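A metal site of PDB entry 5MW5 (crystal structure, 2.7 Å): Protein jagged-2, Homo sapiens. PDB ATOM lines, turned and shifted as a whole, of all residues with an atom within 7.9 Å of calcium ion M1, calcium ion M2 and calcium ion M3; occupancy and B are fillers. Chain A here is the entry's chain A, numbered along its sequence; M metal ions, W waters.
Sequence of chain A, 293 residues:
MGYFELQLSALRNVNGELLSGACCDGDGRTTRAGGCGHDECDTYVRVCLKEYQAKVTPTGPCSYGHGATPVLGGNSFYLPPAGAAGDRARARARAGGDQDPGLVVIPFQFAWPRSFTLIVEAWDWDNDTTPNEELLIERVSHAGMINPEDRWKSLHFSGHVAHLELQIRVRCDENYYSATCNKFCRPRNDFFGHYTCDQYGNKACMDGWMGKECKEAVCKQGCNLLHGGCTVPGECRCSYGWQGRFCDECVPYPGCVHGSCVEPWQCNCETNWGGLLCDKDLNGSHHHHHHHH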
ATOM      1  N   LEU A  18      12.246  -7.744   0.613  1.00  0.00           N
ATOM      2  CA  LEU A  18      11.128  -6.862   0.335  1.00  0.00           C
ATOM      3  C   LEU A  18      11.642  -5.427   0.181  1.00  0.00           C
ATOM      4  O   LEU A  18      12.813  -5.135   0.419  1.00  0.00           O
ATOM      5  CB  LEU A  18      10.066  -6.936   1.439  1.00  0.00           C
ATOM      6  CG  LEU A  18       9.603  -8.323   1.899  1.00  0.00           C
ATOM      7  CD1 LEU A  18       9.931  -8.514   3.363  1.00  0.00           C
ATOM      8  CD2 LEU A  18       8.119  -8.532   1.648  1.00  0.00           C
ATOM      9  N   CYS A  23      13.732  -9.461   5.305  1.00  0.00           N
ATOM     10  CA  CYS A  23      13.527 -10.720   4.625  1.00  0.00           C
ATOM     11  C   CYS A  23      12.043 -11.061   4.606  1.00  0.00           C
ATOM     12  O   CYS A  23      11.291 -10.706   5.525  1.00  0.00           O
ATOM     13  CB  CYS A  23      14.321 -11.841   5.304  1.00  0.00           C
ATOM     14  SG  CYS A  23      16.120 -11.623   5.285  1.00  0.00           S
ATOM     15  N   CYS A  24      11.622 -11.762   3.549  1.00  0.00           N
ATOM     16  CA  CYS A  24      10.207 -12.078   3.379  1.00  0.00           C
ATOM     17  C   CYS A  24       9.684 -12.919   4.538  1.00  0.00           C
ATOM     18  O   CYS A  24       8.744 -12.516   5.248  1.00  0.00           O
ATOM     19  CB  CYS A  24       9.995 -12.799   2.054  1.00  0.00           C
ATOM     20  SG  CYS A  24      10.022 -11.738   0.600  1.00  0.00           S
ATOM     21  N   ASP A  25      10.272 -14.080   4.754  1.00  0.00           N
ATOM     22  CA  ASP A  25       9.838 -14.976   5.816  1.00  0.00           C
ATOM     23  C   ASP A  25      11.006 -15.398   6.699  1.00  0.00           C
ATOM     24  O   ASP A  25      11.192 -14.867   7.787  1.00  0.00           O
ATOM     25  CB  ASP A  25       9.141 -16.198   5.219  1.00  0.00           C
ATOM     26  CG  ASP A  25       7.971 -15.830   4.332  1.00  0.00           C
ATOM     27  OD1 ASP A  25       7.389 -14.744   4.538  1.00  0.00           O
ATOM     28  OD2 ASP A  25       7.626 -16.621   3.429  1.00  0.00           O
ATOM     29  N   HIS A  38      16.023 -19.624   3.881  1.00  0.00           N
ATOM     30  CA  HIS A  38      15.464 -20.575   2.923  1.00  0.00           C
ATOM     31  C   HIS A  38      13.951 -20.521   2.786  1.00  0.00           C
ATOM     32  O   HIS A  38      13.438 -20.952   1.751  1.00  0.00           O
ATOM     33  CB  HIS A  38      15.863 -22.010   3.299  1.00  0.00           C
ATOM     34  CG  HIS A  38      17.173 -22.450   2.705  1.00  0.00           C
ATOM     35  ND1 HIS A  38      17.392 -22.469   1.344  1.00  0.00           N
ATOM     36  CD2 HIS A  38      18.313 -22.874   3.289  1.00  0.00           C
ATOM     37  CE1 HIS A  38      18.626 -22.891   1.118  1.00  0.00           C
ATOM     38  NE2 HIS A  38      19.198 -23.145   2.275  1.00  0.00           N
ATOM     39  N   ASP A  39      13.220 -20.010   3.780  1.00  0.00           N
ATOM     40  CA  ASP A  39      11.784 -19.780   3.633  1.00  0.00           C
ATOM     41  C   ASP A  39      11.585 -18.612   2.672  1.00  0.00           C
ATOM     42  O   ASP A  39      11.710 -17.450   3.059  1.00  0.00           O
ATOM     43  CB  ASP A  39      11.145 -19.521   4.987  1.00  0.00           C
ATOM     44  CG  ASP A  39       9.626 -19.504   4.934  1.00  0.00           C
ATOM     45  OD1 ASP A  39       9.060 -19.721   3.848  1.00  0.00           O
ATOM     46  OD2 ASP A  39       8.997 -19.295   5.993  1.00  0.00           O
ATOM     47  N   GLU A  40      11.293 -18.924   1.409  1.00  0.00           N
ATOM     48  CA  GLU A  40      11.355 -17.929   0.349  1.00  0.00           C
ATOM     49  C   GLU A  40      10.148 -16.998   0.390  1.00  0.00           C
ATOM     50  O   GLU A  40       9.189 -17.200   1.133  1.00  0.00           O
ATOM     51  CB  GLU A  40      11.435 -18.607  -1.016  1.00  0.00           C
ATOM     52  CG  GLU A  40      12.528 -19.652  -1.129  1.00  0.00           C
ATOM     53  CD  GLU A  40      13.296 -19.520  -2.428  1.00  0.00           C
ATOM     54  OE1 GLU A  40      14.381 -20.140  -2.537  1.00  0.00           O
ATOM     55  OE2 GLU A  40      12.835 -18.788  -3.334  1.00  0.00           O
ATOM     56  N   CYS A  41      10.222 -15.969  -0.448  1.00  0.00           N
ATOM     57  CA  CYS A  41       9.066 -15.110  -0.681  1.00  0.00           C
ATOM     58  C   CYS A  41       7.998 -15.891  -1.435  1.00  0.00           C
ATOM     59  O   CYS A  41       8.303 -16.604  -2.401  1.00  0.00           O
ATOM     60  CB  CYS A  41       9.473 -13.868  -1.481  1.00  0.00           C
ATOM     61  SG  CYS A  41      10.859 -12.941  -0.808  1.00  0.00           S
ATOM     62  N   ASP A  42       6.757 -15.784  -0.988  1.00  0.00           N
ATOM     63  CA  ASP A  42       5.625 -16.423  -1.661  1.00  0.00           C
ATOM     64  C   ASP A  42       4.990 -15.351  -2.534  1.00  0.00           C
ATOM     65  O   ASP A  42       4.075 -14.637  -2.122  1.00  0.00           O
ATOM     66  CB  ASP A  42       4.666 -17.018  -0.641  1.00  0.00           C
ATOM     67  CG  ASP A  42       5.400 -17.688   0.524  1.00  0.00           C
ATOM     68  OD1 ASP A  42       6.064 -18.723   0.309  1.00  0.00           O
ATOM     69  OD2 ASP A  42       5.314 -17.164   1.657  1.00  0.00           O
ATOM     70  N   THR A  43       5.480 -15.252  -3.767  1.00  0.00           N
ATOM     71  CA  THR A  43       5.308 -14.063  -4.587  1.00  0.00           C
ATOM     72  C   THR A  43       4.022 -14.119  -5.413  1.00  0.00           C
ATOM     73  O   THR A  43       3.758 -15.111  -6.096  1.00  0.00           O
ATOM     74  CB  THR A  43       6.506 -13.894  -5.521  1.00  0.00           C
ATOM     75  OG1 THR A  43       7.717 -13.862  -4.745  1.00  0.00           O
ATOM     76  CG2 THR A  43       6.395 -12.609  -6.326  1.00  0.00           C
ATOM     77  N   GLY A  73       5.559 -18.356  -7.454  1.00  0.00           N
ATOM     78  CA  GLY A  73       6.825 -18.998  -7.188  1.00  0.00           C
ATOM     79  C   GLY A  73       7.506 -18.395  -5.980  1.00  0.00           C
ATOM     80  O   GLY A  73       6.901 -17.673  -5.187  1.00  0.00           O
ATOM     81  N   GLY A  74       8.791 -18.722  -5.846  1.00  0.00           N
ATOM     82  CA  GLY A  74       9.570 -18.300  -4.704  1.00  0.00           C
ATOM     83  C   GLY A  74      10.246 -16.959  -4.881  1.00  0.00           C
ATOM     84  O   GLY A  74       9.613 -15.905  -4.759  1.00  0.00           O
ATOM     85  N   TRP A 123       4.337  -8.997  -4.219  1.00  0.00           N
ATOM     86  CA  TRP A 123       3.989  -9.147  -2.815  1.00  0.00           C
ATOM     87  C   TRP A 123       4.363 -10.526  -2.314  1.00  0.00           C
ATOM     88  O   TRP A 123       4.258 -11.515  -3.046  1.00  0.00           O
ATOM     89  CB  TRP A 123       2.493  -8.923  -2.580  1.00  0.00           C
ATOM     90  CG  TRP A 123       2.026  -7.517  -2.791  1.00  0.00           C
ATOM     91  CD1 TRP A 123       1.782  -6.912  -3.989  1.00  0.00           C
ATOM     92  CD2 TRP A 123       1.733  -6.545  -1.781  1.00  0.00           C
ATOM     93  NE1 TRP A 123       1.360  -5.625  -3.786  1.00  0.00           N
ATOM     94  CE2 TRP A 123       1.325  -5.371  -2.433  1.00  0.00           C
ATOM     95  CE3 TRP A 123       1.785  -6.557  -0.388  1.00  0.00           C
ATOM     96  CZ2 TRP A 123       0.965  -4.222  -1.749  1.00  0.00           C
ATOM     97  CZ3 TRP A 123       1.425  -5.408   0.296  1.00  0.00           C
ATOM     98  CH2 TRP A 123       1.021  -4.260  -0.381  1.00  0.00           C
ATOM     99  N   ASP A 124       4.783 -10.592  -1.057  1.00  0.00           N
ATOM    100  CA  ASP A 124       4.902 -11.862  -0.338  1.00  0.00           C
ATOM    101  C   ASP A 124       3.601 -12.130   0.401  1.00  0.00           C
ATOM    102  O   ASP A 124       3.116 -11.271   1.155  1.00  0.00           O
ATOM    103  CB  ASP A 124       6.079 -11.841   0.644  1.00  0.00           C
ATOM    104  CG  ASP A 124       6.075 -13.049   1.576  1.00  0.00           C
ATOM    105  OD1 ASP A 124       6.470 -14.146   1.133  1.00  0.00           O
ATOM    106  OD2 ASP A 124       5.701 -12.894   2.757  1.00  0.00           O
ATOM    107  N   TRP A 125       3.030 -13.308   0.174  1.00  0.00           N
ATOM    108  CA  TRP A 125       1.863 -13.765   0.904  1.00  0.00           C
ATOM    109  C   TRP A 125       2.324 -14.509   2.151  1.00  0.00           C
ATOM    110  O   TRP A 125       3.353 -15.189   2.150  1.00  0.00           O
ATOM    111  CB  TRP A 125       0.996 -14.647   0.003  1.00  0.00           C
ATOM    112  CG  TRP A 125      -0.040 -15.446   0.716  1.00  0.00           C
ATOM    113  CD1 TRP A 125      -1.343 -15.109   0.908  1.00  0.00           C
ATOM    114  CD2 TRP A 125       0.138 -16.732   1.315  1.00  0.00           C
ATOM    115  NE1 TRP A 125      -1.996 -16.105   1.599  1.00  0.00           N
ATOM    116  CE2 TRP A 125      -1.099 -17.113   1.857  1.00  0.00           C
ATOM    117  CE3 TRP A 125       1.228 -17.591   1.453  1.00  0.00           C
ATOM    118  CZ2 TRP A 125      -1.274 -18.317   2.527  1.00  0.00           C
ATOM    119  CZ3 TRP A 125       1.056 -18.782   2.113  1.00  0.00           C
ATOM    120  CH2 TRP A 125      -0.189 -19.136   2.649  1.00  0.00           C
ATOM    121  N   ASP A 126       1.548 -14.380   3.240  1.00  0.00           N
ATOM    122  CA  ASP A 126       2.040 -14.766   4.548  1.00  0.00           C
ATOM    123  C   ASP A 126       1.102 -15.605   5.409  1.00  0.00           C
ATOM    124  O   ASP A 126       1.420 -15.859   6.574  1.00  0.00           O
ATOM    125  CB  ASP A 126       2.425 -13.513   5.354  1.00  0.00           C
ATOM    126  CG  ASP A 126       3.916 -13.284   5.402  1.00  0.00           C
ATOM    127  OD1 ASP A 126       4.629 -13.950   4.625  1.00  0.00           O
ATOM    128  OD2 ASP A 126       4.377 -12.459   6.208  1.00  0.00           O
ATOM    129  N   ASN A 127      -0.041 -16.049   4.863  1.00  0.00           N
ATOM    130  CA  ASN A 127      -1.030 -16.816   5.629  1.00  0.00           C
ATOM    131  C   ASN A 127      -1.483 -16.028   6.866  1.00  0.00           C
ATOM    132  O   ASN A 127      -1.197 -16.377   8.015  1.00  0.00           O
ATOM    133  CB  ASN A 127      -0.486 -18.195   6.012  1.00  0.00           C
ATOM    134  CG  ASN A 127      -1.472 -19.020   6.818  1.00  0.00           C
ATOM    135  OD1 ASN A 127      -2.683 -18.817   6.744  1.00  0.00           O
ATOM    136  ND2 ASN A 127      -0.959 -19.965   7.605  1.00  0.00           N
ATOM    137  N   ASN A 132      -1.527  -6.655   5.754  1.00  0.00           N
ATOM    138  CA  ASN A 132      -0.220  -6.116   6.140  1.00  0.00           C
ATOM    139  C   ASN A 132       0.443  -5.531   4.896  1.00  0.00           C
ATOM    140  O   ASN A 132       0.905  -6.264   4.022  1.00  0.00           O
ATOM    141  CB  ASN A 132       0.632  -7.218   6.764  1.00  0.00           C
ATOM    142  CG  ASN A 132       1.995  -6.723   7.222  1.00  0.00           C
ATOM    143  OD1 ASN A 132       2.288  -5.526   7.189  1.00  0.00           O
ATOM    144  ND2 ASN A 132       2.841  -7.657   7.649  1.00  0.00           N
ATOM    145  N   GLU A 134       3.226  -3.876   4.715  1.00  0.00           N
ATOM    146  CA  GLU A 134       4.687  -3.926   4.796  1.00  0.00           C
ATOM    147  C   GLU A 134       5.257  -5.082   3.974  1.00  0.00           C
ATOM    148  O   GLU A 134       6.473  -5.157   3.756  1.00  0.00           O
ATOM    149  CB  GLU A 134       5.124  -4.033   6.262  1.00  0.00           C
ATOM    150  CG  GLU A 134       6.624  -3.833   6.487  1.00  0.00           C
ATOM    151  CD  GLU A 134       6.954  -3.307   7.868  1.00  0.00           C
ATOM    152  OE1 GLU A 134       7.726  -2.333   7.957  1.00  0.00           O
ATOM    153  OE2 GLU A 134       6.461  -3.881   8.862  1.00  0.00           O
ATOM    154  N   LEU A 135       4.393  -5.987   3.507  1.00  0.00           N
ATOM    155  CA  LEU A 135       4.804  -7.152   2.749  1.00  0.00           C
ATOM    156  C   LEU A 135       4.973  -6.865   1.263  1.00  0.00           C
ATOM    157  O   LEU A 135       4.817  -7.783   0.437  1.00  0.00           O
ATOM    158  CB  LEU A 135       3.794  -8.280   2.951  1.00  0.00           C
ATOM    159  CG  LEU A 135       3.710  -8.864   4.369  1.00  0.00           C
ATOM    160  CD1 LEU A 135       2.567  -9.865   4.462  1.00  0.00           C
ATOM    161  CD2 LEU A 135       5.025  -9.514   4.742  1.00  0.00           C
HETATM  162 CA    CA M   1       5.674 -15.286   3.022  1.00  0.00          CA
HETATM  163 CA    CA M   2       7.620 -18.671   2.202  1.00  0.00          CA
HETATM  164 CA    CA M   3       6.450 -12.645   5.061  1.00  0.00          CA
HETATM  165  O   HOH W   1       8.427 -20.588   0.932  1.00  0.00           O
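Calcium ion M2 is bound by the side-chain carboxylate (OD2) of Asp 25 (2.4 Å), the backbone carbonyl oxygen (O) of Glu 40 (2.4 Å), the side-chain carboxylate (OD1) of Asp 39 (2.4 Å), water W1 (2.4 Å), the side-chain carboxylate (OD1) of Asp 42 (2.5 Å) and the side-chain carboxylate (OD2) of Asp 42 (2.8 Å). Calcium ion M2 has six donor atoms within binding distance.
Calcium ion M3 is bound by OD1 of Asp 126 (2.3 Å), O of Cys 24 (2.3 Å), OD1 of Asp 25 (2.4 Å), OD2 of Asp 126 (2.4 Å) and OD2 of Asp 124 (2.4 Å).
The backbone NH (N) of Asp 124 sits at hydrogen-bond distance from the backbone carbonyl oxygen (O) of Leu 135 (3.2 Å). SG of Cys 24 forms a disulfide with SG of Cys 41 (2.0 Å).
Leu 135 touches calcium ion M3 (CD2 to CA, 3.5 Å). Of the 20 residues printed, 5 come within 4 Å of calcium ion M3. Along chain A the residues within 4 Å of calcium ion M3 span positions 24 to 135. The nearest printed residue that does not touch calcium ion M3 is Trp 125 (5.0 Å).
The nearest printed residue that does not touch calcium ion M1 is Glu 40 (4.4 Å).
Calcium ion M1 is bound by OD1 of Asp 126 (2.3 Å), OD1 of Asp 124 (2.3 Å), OD2 of Asp 42 (2.3 Å), OD1 of Asp 25 (2.4 Å), OD2 of Asp 25 (2.4 Å), OD2 of Asp 124 (2.4 Å) and O of Trp 125 (2.5 Å).
Within 4 Å of calcium ion M2: Asp 25, Asp 39, Glu 40 and Asp 42.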
